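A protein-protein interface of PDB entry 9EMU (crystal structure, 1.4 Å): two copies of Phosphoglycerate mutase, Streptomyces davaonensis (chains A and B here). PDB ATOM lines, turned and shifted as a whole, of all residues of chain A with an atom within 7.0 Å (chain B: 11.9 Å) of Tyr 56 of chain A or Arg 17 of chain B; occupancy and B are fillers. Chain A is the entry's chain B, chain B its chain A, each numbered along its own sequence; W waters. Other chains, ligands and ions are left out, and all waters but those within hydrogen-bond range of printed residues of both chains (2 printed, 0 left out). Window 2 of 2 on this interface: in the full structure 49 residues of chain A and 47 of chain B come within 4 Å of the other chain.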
ATOM      1  N   SER A  49     -11.549  -6.893   7.673  1.00  0.00           N
ATOM      2  CA  SER A  49     -10.764  -6.004   6.831  1.00  0.00           C
ATOM      3  C   SER A  49     -11.263  -4.579   6.960  1.00  0.00           C
ATOM      4  O   SER A  49     -10.880  -3.724   6.147  1.00  0.00           O
ATOM      5  CB  SER A  49     -10.850  -6.433   5.360  1.00  0.00           C
ATOM      6  OG  SER A  49     -12.219  -6.528   4.994  1.00  0.00           O
ATOM      7  N   THR A  51     -11.740  -2.767  10.285  1.00  0.00           N
ATOM      8  CA  THR A  51     -11.238  -1.954  11.388  1.00  0.00           C
ATOM      9  C   THR A  51     -10.185  -1.000  10.849  1.00  0.00           C
ATOM     10  O   THR A  51      -9.241  -1.425  10.178  1.00  0.00           O
ATOM     11  CB  THR A  51     -10.613  -2.839  12.463  1.00  0.00           C
ATOM     12  OG1 THR A  51     -11.593  -3.755  12.954  1.00  0.00           O
ATOM     13  CG2 THR A  51     -10.114  -1.992  13.629  1.00  0.00           C
ATOM     14  N   GLY A  52     -10.360   0.291  11.112  1.00  0.00           N
ATOM     15  CA  GLY A  52      -9.428   1.269  10.587  1.00  0.00           C
ATOM     16  C   GLY A  52      -9.616   1.629   9.129  1.00  0.00           C
ATOM     17  O   GLY A  52      -8.757   2.321   8.570  1.00  0.00           O
ATOM     18  N   LEU A  53     -10.713   1.194   8.500  1.00  0.00           N
ATOM     19  CA  LEU A  53     -10.941   1.511   7.094  1.00  0.00           C
ATOM     20  C   LEU A  53     -11.039   3.012   6.865  1.00  0.00           C
ATOM     21  O   LEU A  53     -10.651   3.497   5.801  1.00  0.00           O
ATOM     22  CB  LEU A  53     -12.207   0.808   6.585  1.00  0.00           C
ATOM     23  CG  LEU A  53     -12.459   0.906   5.065  1.00  0.00           C
ATOM     24  CD1 LEU A  53     -11.481   0.038   4.279  1.00  0.00           C
ATOM     25  CD2 LEU A  53     -13.901   0.534   4.719  1.00  0.00           C
ATOM     26  N   GLU A  54     -11.535   3.762   7.856  1.00  0.00           N
ATOM     27  CA  GLU A  54     -11.669   5.207   7.692  1.00  0.00           C
ATOM     28  C   GLU A  54     -10.334   5.873   7.389  1.00  0.00           C
ATOM     29  O   GLU A  54     -10.305   6.923   6.735  1.00  0.00           O
ATOM     30  CB  GLU A  54     -12.323   5.831   8.932  1.00  0.00           C
ATOM     31  CG  GLU A  54     -11.581   5.599  10.244  1.00  0.00           C
ATOM     32  CD  GLU A  54     -11.823   4.217  10.839  1.00  0.00           C
ATOM     33  OE1 GLU A  54     -12.574   3.420  10.233  1.00  0.00           O
ATOM     34  OE2 GLU A  54     -11.257   3.930  11.917  1.00  0.00           O
ATOM     35  N   ASP A  55      -9.226   5.282   7.840  1.00  0.00           N
ATOM     36  CA  ASP A  55      -7.897   5.854   7.658  1.00  0.00           C
ATOM     37  C   ASP A  55      -7.073   5.156   6.581  1.00  0.00           C
ATOM     38  O   ASP A  55      -5.899   5.496   6.397  1.00  0.00           O
ATOM     39  CB  ASP A  55      -7.120   5.824   8.981  1.00  0.00           C
ATOM     40  CG  ASP A  55      -7.791   6.636  10.075  1.00  0.00           C
ATOM     41  OD1 ASP A  55      -8.363   7.699   9.759  1.00  0.00           O
ATOM     42  OD2 ASP A  55      -7.745   6.212  11.249  1.00  0.00           O
ATOM     43  N   TYR A  56      -7.654   4.202   5.857  1.00  0.00           N
ATOM     44  CA  TYR A  56      -6.892   3.306   4.997  1.00  0.00           C
ATOM     45  C   TYR A  56      -6.490   4.005   3.709  1.00  0.00           C
ATOM     46  O   TYR A  56      -7.307   4.678   3.079  1.00  0.00           O
ATOM     47  CB  TYR A  56      -7.789   2.122   4.654  1.00  0.00           C
ATOM     48  CG  TYR A  56      -7.154   0.971   3.918  1.00  0.00           C
ATOM     49  CD1 TYR A  56      -6.001   0.347   4.398  1.00  0.00           C
ATOM     50  CD2 TYR A  56      -7.739   0.473   2.765  1.00  0.00           C
ATOM     51  CE1 TYR A  56      -5.456  -0.747   3.730  1.00  0.00           C
ATOM     52  CE2 TYR A  56      -7.202  -0.614   2.092  1.00  0.00           C
ATOM     53  CZ  TYR A  56      -6.062  -1.216   2.575  1.00  0.00           C
ATOM     54  OH  TYR A  56      -5.543  -2.308   1.912  1.00  0.00           O
ATOM     55  N   ASP A  57      -5.230   3.805   3.297  1.00  0.00           N
ATOM     56  CA  ASP A  57      -4.666   4.426   2.105  1.00  0.00           C
ATOM     57  C   ASP A  57      -4.716   3.536   0.868  1.00  0.00           C
ATOM     58  O   ASP A  57      -4.418   4.015  -0.232  1.00  0.00           O
ATOM     59  CB  ASP A  57      -3.213   4.876   2.369  1.00  0.00           C
ATOM     60  CG  ASP A  57      -2.317   3.737   2.868  1.00  0.00           C
ATOM     61  OD1 ASP A  57      -2.851   2.710   3.341  1.00  0.00           O
ATOM     62  OD2 ASP A  57      -1.071   3.877   2.795  1.00  0.00           O
ATOM     63  N   GLY A  58      -5.078   2.263   1.024  1.00  0.00           N
ATOM     64  CA  GLY A  58      -5.258   1.349  -0.093  1.00  0.00           C
ATOM     65  C   GLY A  58      -6.608   1.527  -0.758  1.00  0.00           C
ATOM     66  O   GLY A  58      -7.335   2.489  -0.515  1.00  0.00           O
ATOM     67  N   ASP A  59      -6.932   0.579  -1.637  1.00  0.00           N
ATOM     68  CA  ASP A  59      -8.249   0.509  -2.258  1.00  0.00           C
ATOM     69  C   ASP A  59      -9.277   0.176  -1.180  1.00  0.00           C
ATOM     70  O   ASP A  59      -9.283  -0.952  -0.678  1.00  0.00           O
ATOM     71  CB  ASP A  59      -8.225  -0.572  -3.340  1.00  0.00           C
ATOM     72  CG  ASP A  59      -9.491  -0.605  -4.178  1.00  0.00           C
ATOM     73  OD1 ASP A  59     -10.525  -0.053  -3.752  1.00  0.00           O
ATOM     74  OD2 ASP A  59      -9.447  -1.205  -5.268  1.00  0.00           O
ATOM     75  N   PRO A  60     -10.143   1.114  -0.787  1.00  0.00           N
ATOM     76  CA  PRO A  60     -11.050   0.851   0.336  1.00  0.00           C
ATOM     77  C   PRO A  60     -12.128  -0.151   0.002  1.00  0.00           C
ATOM     78  O   PRO A  60     -12.733  -0.716   0.922  1.00  0.00           O
ATOM     79  CB  PRO A  60     -11.647   2.231   0.629  1.00  0.00           C
ATOM     80  CG  PRO A  60     -11.644   2.905  -0.719  1.00  0.00           C
ATOM     81  CD  PRO A  60     -10.375   2.439  -1.394  1.00  0.00           C
ATOM     82  N   ARG A  61     -12.395  -0.383  -1.276  1.00  0.00           N
ATOM     83  CA  ARG A  61     -13.334  -1.420  -1.675  1.00  0.00           C
ATOM     84  C   ARG A  61     -12.687  -2.784  -1.828  1.00  0.00           C
ATOM     85  O   ARG A  61     -13.406  -3.770  -2.010  1.00  0.00           O
ATOM     86  CB  ARG A  61     -14.026  -1.037  -2.985  1.00  0.00           C
ATOM     87  CG  ARG A  61     -14.810   0.231  -2.887  1.00  0.00           C
ATOM     88  CD  ARG A  61     -15.416   0.561  -4.242  1.00  0.00           C
ATOM     89  NE  ARG A  61     -16.143   1.817  -4.204  1.00  0.00           N
ATOM     90  CZ  ARG A  61     -15.588   3.003  -4.406  1.00  0.00           C
ATOM     91  NH1 ARG A  61     -14.305   3.122  -4.706  1.00  0.00           N
ATOM     92  NH2 ARG A  61     -16.336   4.095  -4.295  1.00  0.00           N
ATOM     93  N   ASP A  62     -11.358  -2.876  -1.747  1.00  0.00           N
ATOM     94  CA  ASP A  62     -10.661  -4.166  -1.770  1.00  0.00           C
ATOM     95  C   ASP A  62      -9.552  -4.150  -0.720  1.00  0.00           C
ATOM     96  O   ASP A  62      -8.371  -4.284  -1.043  1.00  0.00           O
ATOM     97  CB  ASP A  62     -10.093  -4.405  -3.169  1.00  0.00           C
ATOM     98  CG  ASP A  62      -9.590  -5.825  -3.400  1.00  0.00           C
ATOM     99  OD1 ASP A  62      -9.808  -6.738  -2.567  1.00  0.00           O
ATOM    100  OD2 ASP A  62      -8.976  -6.026  -4.472  1.00  0.00           O
ATOM    101  N   PRO A  63      -9.906  -4.003   0.558  1.00  0.00           N
ATOM    102  CA  PRO A  63      -8.879  -3.903   1.601  1.00  0.00           C
ATOM    103  C   PRO A  63      -8.225  -5.239   1.935  1.00  0.00           C
ATOM    104  O   PRO A  63      -8.814  -6.321   1.803  1.00  0.00           O
ATOM    105  CB  PRO A  63      -9.668  -3.386   2.811  1.00  0.00           C
ATOM    106  CG  PRO A  63     -11.069  -3.967   2.585  1.00  0.00           C
ATOM    107  CD  PRO A  63     -11.268  -3.852   1.111  1.00  0.00           C
ATOM    108  N   ALA A  64      -6.979  -5.143   2.388  1.00  0.00           N
ATOM    109  CA  ALA A  64      -6.339  -6.269   3.047  1.00  0.00           C
ATOM    110  C   ALA A  64      -6.977  -6.498   4.420  1.00  0.00           C
ATOM    111  O   ALA A  64      -7.788  -5.701   4.906  1.00  0.00           O
ATOM    112  CB  ALA A  64      -4.848  -5.995   3.233  1.00  0.00           C
ATOM    113  N   LEU A  65      -6.580  -7.586   5.063  1.00  0.00           N
ATOM    114  CA  LEU A  65      -7.056  -7.804   6.421  1.00  0.00           C
ATOM    115  C   LEU A  65      -6.476  -6.753   7.363  1.00  0.00           C
ATOM    116  O   LEU A  65      -5.346  -6.284   7.201  1.00  0.00           O
ATOM    117  CB  LEU A  65      -6.648  -9.186   6.928  1.00  0.00           C
ATOM    118  CG  LEU A  65      -7.258 -10.395   6.210  1.00  0.00           C
ATOM    119  CD1 LEU A  65      -6.827 -11.666   6.928  1.00  0.00           C
ATOM    120  CD2 LEU A  65      -8.778 -10.307   6.130  1.00  0.00           C
ATOM    121  N   HIS A  94      -8.732  -9.344  -1.914  1.00  0.00           N
ATOM    122  CA  HIS A  94      -7.612  -9.529  -1.000  1.00  0.00           C
ATOM    123  C   HIS A  94      -8.056 -10.123   0.330  1.00  0.00           C
ATOM    124  O   HIS A  94      -7.408 -11.037   0.853  1.00  0.00           O
ATOM    125  CB  HIS A  94      -6.926  -8.186  -0.746  1.00  0.00           C
ATOM    126  CG  HIS A  94      -6.231  -7.611  -1.938  1.00  0.00           C
ATOM    127  ND1 HIS A  94      -5.256  -8.293  -2.629  1.00  0.00           N
ATOM    128  CD2 HIS A  94      -6.338  -6.401  -2.529  1.00  0.00           C
ATOM    129  CE1 HIS A  94      -4.802  -7.535  -3.614  1.00  0.00           C
ATOM    130  NE2 HIS A  94      -5.446  -6.381  -3.576  1.00  0.00           N
ATOM    131  N   TRP A 124     -21.912   0.893  -2.611  1.00  0.00           N
ATOM    132  CA  TRP A 124     -20.577   1.466  -2.537  1.00  0.00           C
ATOM    133  C   TRP A 124     -19.741   1.107  -3.759  1.00  0.00           C
ATOM    134  O   TRP A 124     -18.986   1.949  -4.262  1.00  0.00           O
ATOM    135  CB  TRP A 124     -19.881   1.044  -1.254  1.00  0.00           C
ATOM    136  CG  TRP A 124     -18.655   1.870  -1.025  1.00  0.00           C
ATOM    137  CD1 TRP A 124     -18.409   3.130  -1.500  1.00  0.00           C
ATOM    138  CD2 TRP A 124     -17.509   1.494  -0.274  1.00  0.00           C
ATOM    139  NE1 TRP A 124     -17.176   3.561  -1.081  1.00  0.00           N
ATOM    140  CE2 TRP A 124     -16.602   2.573  -0.326  1.00  0.00           C
ATOM    141  CE3 TRP A 124     -17.157   0.349   0.442  1.00  0.00           C
ATOM    142  CZ2 TRP A 124     -15.369   2.535   0.306  1.00  0.00           C
ATOM    143  CZ3 TRP A 124     -15.942   0.317   1.071  1.00  0.00           C
ATOM    144  CH2 TRP A 124     -15.060   1.401   1.003  1.00  0.00           C
ATOM    145  N   SER A 130     -24.217   4.269   1.026  1.00  0.00           N
ATOM    146  CA  SER A 130     -24.871   3.078   1.541  1.00  0.00           C
ATOM    147  C   SER A 130     -26.114   3.463   2.335  1.00  0.00           C
ATOM    148  O   SER A 130     -26.216   4.574   2.870  1.00  0.00           O
ATOM    149  CB  SER A 130     -23.906   2.296   2.423  1.00  0.00           C
ATOM    150  OG  SER A 130     -22.794   1.860   1.663  1.00  0.00           O
ATOM    151  N   SER B  14     -15.523  12.270   2.552  1.00  0.00           N
ATOM    152  CA  SER B  14     -15.757  10.832   2.445  1.00  0.00           C
ATOM    153  C   SER B  14     -16.001  10.405   1.000  1.00  0.00           C
ATOM    154  O   SER B  14     -16.700  11.079   0.248  1.00  0.00           O
ATOM    155  CB  SER B  14     -16.940  10.404   3.327  1.00  0.00           C
ATOM    156  OG  SER B  14     -17.198   9.005   3.228  1.00  0.00           O
ATOM    157  N   ASP B  15     -15.416   9.270   0.620  1.00  0.00           N
ATOM    158  CA  ASP B  15     -15.611   8.684  -0.698  1.00  0.00           C
ATOM    159  C   ASP B  15     -16.688   7.600  -0.697  1.00  0.00           C
ATOM    160  O   ASP B  15     -16.723   6.761  -1.605  1.00  0.00           O
ATOM    161  CB  ASP B  15     -14.288   8.125  -1.226  1.00  0.00           C
ATOM    162  CG  ASP B  15     -13.701   7.027  -0.330  1.00  0.00           C
ATOM    163  OD1 ASP B  15     -14.318   6.643   0.689  1.00  0.00           O
ATOM    164  OD2 ASP B  15     -12.601   6.537  -0.651  1.00  0.00           O
ATOM    165  N   GLY B  16     -17.556   7.594   0.311  1.00  0.00           N
ATOM    166  CA  GLY B  16     -18.546   6.549   0.477  1.00  0.00           C
ATOM    167  C   GLY B  16     -18.227   5.546   1.563  1.00  0.00           C
ATOM    168  O   GLY B  16     -19.120   4.790   1.961  1.00  0.00           O
ATOM    169  N   ARG B  17     -16.985   5.511   2.056  1.00  0.00           N
ATOM    170  CA  ARG B  17     -16.650   4.517   3.072  1.00  0.00           C
ATOM    171  C   ARG B  17     -17.320   4.822   4.401  1.00  0.00           C
ATOM    172  O   ARG B  17     -17.599   3.901   5.172  1.00  0.00           O
ATOM    173  CB  ARG B  17     -15.141   4.404   3.255  1.00  0.00           C
ATOM    174  CG  ARG B  17     -14.500   5.606   3.933  1.00  0.00           C
ATOM    175  CD  ARG B  17     -12.988   5.438   4.001  1.00  0.00           C
ATOM    176  NE  ARG B  17     -12.348   5.585   2.697  1.00  0.00           N
ATOM    177  CZ  ARG B  17     -11.047   5.421   2.485  1.00  0.00           C
ATOM    178  NH1 ARG B  17     -10.234   5.025   3.455  1.00  0.00           N
ATOM    179  NH2 ARG B  17     -10.546   5.672   1.277  1.00  0.00           N
ATOM    180  N   GLU B  18     -17.602   6.091   4.686  1.00  0.00           N
ATOM    181  CA  GLU B  18     -18.210   6.427   5.969  1.00  0.00           C
ATOM    182  C   GLU B  18     -19.637   5.897   6.065  1.00  0.00           C
ATOM    183  O   GLU B  18     -20.013   5.287   7.074  1.00  0.00           O
ATOM    184  CB  GLU B  18     -18.157   7.938   6.203  1.00  0.00           C
ATOM    185  CG  GLU B  18     -16.746   8.459   6.448  1.00  0.00           C
ATOM    186  CD  GLU B  18     -16.054   7.770   7.613  1.00  0.00           C
ATOM    187  OE1 GLU B  18     -16.736   7.440   8.607  1.00  0.00           O
ATOM    188  OE2 GLU B  18     -14.825   7.554   7.530  1.00  0.00           O
ATOM    189  N   SER B  19     -20.449   6.101   5.023  1.00  0.00           N
ATOM    190  CA  SER B  19     -21.790   5.530   5.073  1.00  0.00           C
ATOM    191  C   SER B  19     -21.741   4.010   5.044  1.00  0.00           C
ATOM    192  O   SER B  19     -22.537   3.349   5.724  1.00  0.00           O
ATOM    193  CB  SER B  19     -22.678   6.070   3.950  1.00  0.00           C
ATOM    194  OG  SER B  19     -22.264   5.598   2.681  1.00  0.00           O
ATOM    195  N   PHE B  20     -20.813   3.439   4.272  1.00  0.00           N
ATOM    196  CA  PHE B  20     -20.654   1.991   4.269  1.00  0.00           C
ATOM    197  C   PHE B  20     -20.396   1.465   5.677  1.00  0.00           C
ATOM    198  O   PHE B  20     -21.039   0.504   6.122  1.00  0.00           O
ATOM    199  CB  PHE B  20     -19.529   1.601   3.311  1.00  0.00           C
ATOM    200  CG  PHE B  20     -19.212   0.135   3.307  1.00  0.00           C
ATOM    201  CD1 PHE B  20     -20.068  -0.775   2.701  1.00  0.00           C
ATOM    202  CD2 PHE B  20     -18.029  -0.330   3.857  1.00  0.00           C
ATOM    203  CE1 PHE B  20     -19.766  -2.126   2.677  1.00  0.00           C
ATOM    204  CE2 PHE B  20     -17.719  -1.685   3.828  1.00  0.00           C
ATOM    205  CZ  PHE B  20     -18.591  -2.577   3.241  1.00  0.00           C
ATOM    206  N   LEU B  21     -19.464   2.097   6.399  1.00  0.00           N
ATOM    207  CA  LEU B  21     -19.143   1.657   7.754  1.00  0.00           C
ATOM    208  C   LEU B  21     -20.321   1.848   8.703  1.00  0.00           C
ATOM    209  O   LEU B  21     -20.588   0.987   9.542  1.00  0.00           O
ATOM    210  CB  LEU B  21     -17.905   2.395   8.255  1.00  0.00           C
ATOM    211  CG  LEU B  21     -16.592   1.994   7.596  1.00  0.00           C
ATOM    212  CD1 LEU B  21     -15.522   3.002   7.961  1.00  0.00           C
ATOM    213  CD2 LEU B  21     -16.211   0.594   8.033  1.00  0.00           C
ATOM    214  N   GLU B  22     -21.036   2.970   8.594  1.00  0.00           N
ATOM    215  CA  GLU B  22     -22.142   3.227   9.505  1.00  0.00           C
ATOM    216  C   GLU B  22     -23.274   2.238   9.272  1.00  0.00           C
ATOM    217  O   GLU B  22     -23.843   1.695  10.232  1.00  0.00           O
ATOM    218  CB  GLU B  22     -22.630   4.668   9.329  1.00  0.00           C
ATOM    219  CG  GLU B  22     -23.844   5.041  10.181  1.00  0.00           C
ATOM    220  CD  GLU B  22     -23.552   5.069  11.681  1.00  0.00           C
ATOM    221  OE1 GLU B  22     -22.365   5.001  12.070  1.00  0.00           O
ATOM    222  OE2 GLU B  22     -24.516   5.160  12.472  1.00  0.00           O
ATOM    223  N   VAL B  23     -23.588   1.962   8.004  1.00  0.00           N
ATOM    224  CA  VAL B  23     -24.624   0.977   7.692  1.00  0.00           C
ATOM    225  C   VAL B  23     -24.212  -0.404   8.180  1.00  0.00           C
ATOM    226  O   VAL B  23     -25.010  -1.115   8.797  1.00  0.00           O
ATOM    227  CB  VAL B  23     -24.987   0.993   6.193  1.00  0.00           C
ATOM    228  CG1 VAL B  23     -25.923  -0.161   5.854  1.00  0.00           C
ATOM    229  CG2 VAL B  23     -25.646   2.319   5.816  1.00  0.00           C
ATOM    230  N   MET B  24     -22.955  -0.794   7.940  1.00  0.00           N
ATOM    231  CA  MET B  24     -22.480  -2.085   8.429  1.00  0.00           C
ATOM    232  C   MET B  24     -22.629  -2.189   9.944  1.00  0.00           C
ATOM    233  O   MET B  24     -23.072  -3.221  10.465  1.00  0.00           O
ATOM    234  CB  MET B  24     -21.024  -2.280   8.009  1.00  0.00           C
ATOM    235  CG  MET B  24     -20.319  -3.445   8.685  1.00  0.00           C
ATOM    236  SD  MET B  24     -18.571  -3.528   8.234  1.00  0.00           S
ATOM    237  CE  MET B  24     -18.705  -3.811   6.472  1.00  0.00           C
ATOM    238  N   ARG B  25     -22.258  -1.136  10.669  1.00  0.00           N
ATOM    239  CA  ARG B  25     -22.431  -1.148  12.120  1.00  0.00           C
ATOM    240  C   ARG B  25     -23.899  -1.337  12.504  1.00  0.00           C
ATOM    241  O   ARG B  25     -24.224  -2.131  13.402  1.00  0.00           O
ATOM    242  CB  ARG B  25     -21.868   0.137  12.729  1.00  0.00           C
ATOM    243  CG  ARG B  25     -21.706   0.052  14.241  1.00  0.00           C
ATOM    244  CD  ARG B  25     -21.209   1.350  14.836  1.00  0.00           C
ATOM    245  NE  ARG B  25     -22.195   2.408  14.675  1.00  0.00           N
ATOM    246  CZ  ARG B  25     -23.254   2.565  15.457  1.00  0.00           C
ATOM    247  NH1 ARG B  25     -23.492   1.749  16.471  1.00  0.00           N
ATOM    248  NH2 ARG B  25     -24.094   3.566  15.216  1.00  0.00           N
ATOM    249  N   SER B  26     -24.801  -0.606  11.840  1.00  0.00           N
ATOM    250  CA  SER B  26     -26.223  -0.694  12.167  1.00  0.00           C
ATOM    251  C   SER B  26     -26.781  -2.074  11.860  1.00  0.00           C
ATOM    252  O   SER B  26     -27.631  -2.583  12.606  1.00  0.00           O
ATOM    253  CB  SER B  26     -26.999   0.359  11.382  1.00  0.00           C
ATOM    254  OG  SER B  26     -26.622   1.652  11.790  1.00  0.00           O
HETATM  255  O   HOH W   1      -7.897   5.039   0.257  1.00  0.00           O
HETATM  256  O   HOH W   2     -21.234   3.657   0.387  1.00  0.00           O
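No position is printed for both chains.
O of Asp 15 of chain B sits at hydrogen-bond distance from NE1 of Trp 124 of chain A (3.3 Å). The guanidinium group (NH1) of Arg 17 of chain B lies within hydrogen-bond range of the backbone carbonyl oxygen (O) of Leu 53 of chain A. NH1 of Arg 17 of chain B is in hydrogen-bond range of O of Tyr 56 of chain A. N of Ser 130 of chain A is in hydrogen-bond range of OG of Ser 19 of chain B.
The side-chain hydroxyl of Ser 14 of chain B is in hydrogen-bond range of the backbone NH of Gly 16 of chain B (3.3 Å). The side-chain hydroxyl (OG) of Ser 14 of chain B sits at hydrogen-bond distance from the backbone NH (N) of Glu 18 of chain B. OD2 of Asp 15 of chain B lies within salt-bridge range of NH2 of Arg 17 of chain B, 2.9 Å away. The backbone carbonyl oxygen of Gly 16 of chain B lies within hydrogen-bond range of the side-chain hydroxyl of Ser 19 of chain B, at 3.3 Å. N of Ala 64 of chain A sits at hydrogen-bond distance from OH of Tyr 56 of chain A, at 3.2 Å. The side-chain carboxylate (OD1) of Asp 59 of chain A lies within hydrogen-bond range of the backbone NH (N) of Arg 61 of chain A (3.1 Å).
O of Glu 54 of chain A touches NH1 of Arg 17 of chain B, 3.8 Å away. Glu 54 of chain A touches Glu 18 of chain B. Glu 54 of chain A touches Leu 21 of chain B (OE1 to CD1, 3.7 Å). Asp 15 of chain B touches Pro 60 of chain A. Arg 17 of chain B touches Pro 60 of chain A. O of Asp 15 of chain B touches NH2 of Arg 61 of chain A (3.8 Å). NE1 of Trp 124 of chain A touches C of Gly 16 of chain B (3.5 Å). CG of Phe 20 of chain B touches CE3 of Trp 124 of chain A (3.5 Å). CA of Phe 20 of chain B touches OG of Ser 130 of chain A (3.4 Å). Val 23 of chain B touches Ser 130 of chain A (CG2 to C, 3.7 Å).
Leu 53 of chain A touches just one residue of chain B: Arg 17 (2.8 Å). Glu 54 of chain A touches three residues of chain B. No residue of chain B comes within 4 Å of Asp 55 of chain A. No residue of chain B comes within 4 Å of Asp 57 of chain A. No residue of chain B comes within 4 Å of Gly 58 of chain A. No residue of chain B comes within 4 Å of Asp 59 of chain A. Pro 60 of chain A touches two residues of chain B. Of the printed residues of chain B, Arg 61 of chain A touches Asp 15. Asp 62 of chain A touches none of the printed residues of chain B. Ala 64 of chain A touches none of the printed residues of chain B. Printed residues of chain A within 4 Å of Asp 15 of chain B: Pro 60, Arg 61 and Trp 124. Arg 17 of chain B touches five residues of chain A. The nearest residue of chain A that does not touch Arg 17 of chain B is Asp 55 of chain A (4.4 Å). The nearest printed residue of chain A that does not touch Leu 21 of chain B is Leu 53 of chain A (4.04 Å).
Printed residues of chain B that touch a printed residue of chain A: Asp 15, Gly 16, Arg 17, Glu 18, Ser 19, Phe 20, Leu 21 and Val 23. Of the 19 printed residues of chain A, 7 touch a printed residue of chain B. Printed residues of chain A that touch a printed residue of chain B: Leu 53, Glu 54, Tyr 56, Pro 60, Arg 61, Trp 124 and Ser 130. Among the printed residues, 15 pairs touch across the chains. Among the printed residues, no Asp or Glu carboxylate lies within 4 Å of a Lys or Arg side-chain nitrogen of the other chain.
Water W2 lies within hydrogen-bond range of the side-chain hydroxyl of Ser 130 of chain A (2.7 Å), the backbone carbonyl oxygen of Gly 16 of chain B (2.9 Å) and the side-chain hydroxyl of Ser 19 of chain B (3.2 Å). Water W1 lies within hydrogen-bond range of O of Gly 58 of chain A (2.7 Å), O of Tyr 56 of chain A (2.9 Å) and NH2 of Arg 17 of chain B (2.9 Å).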
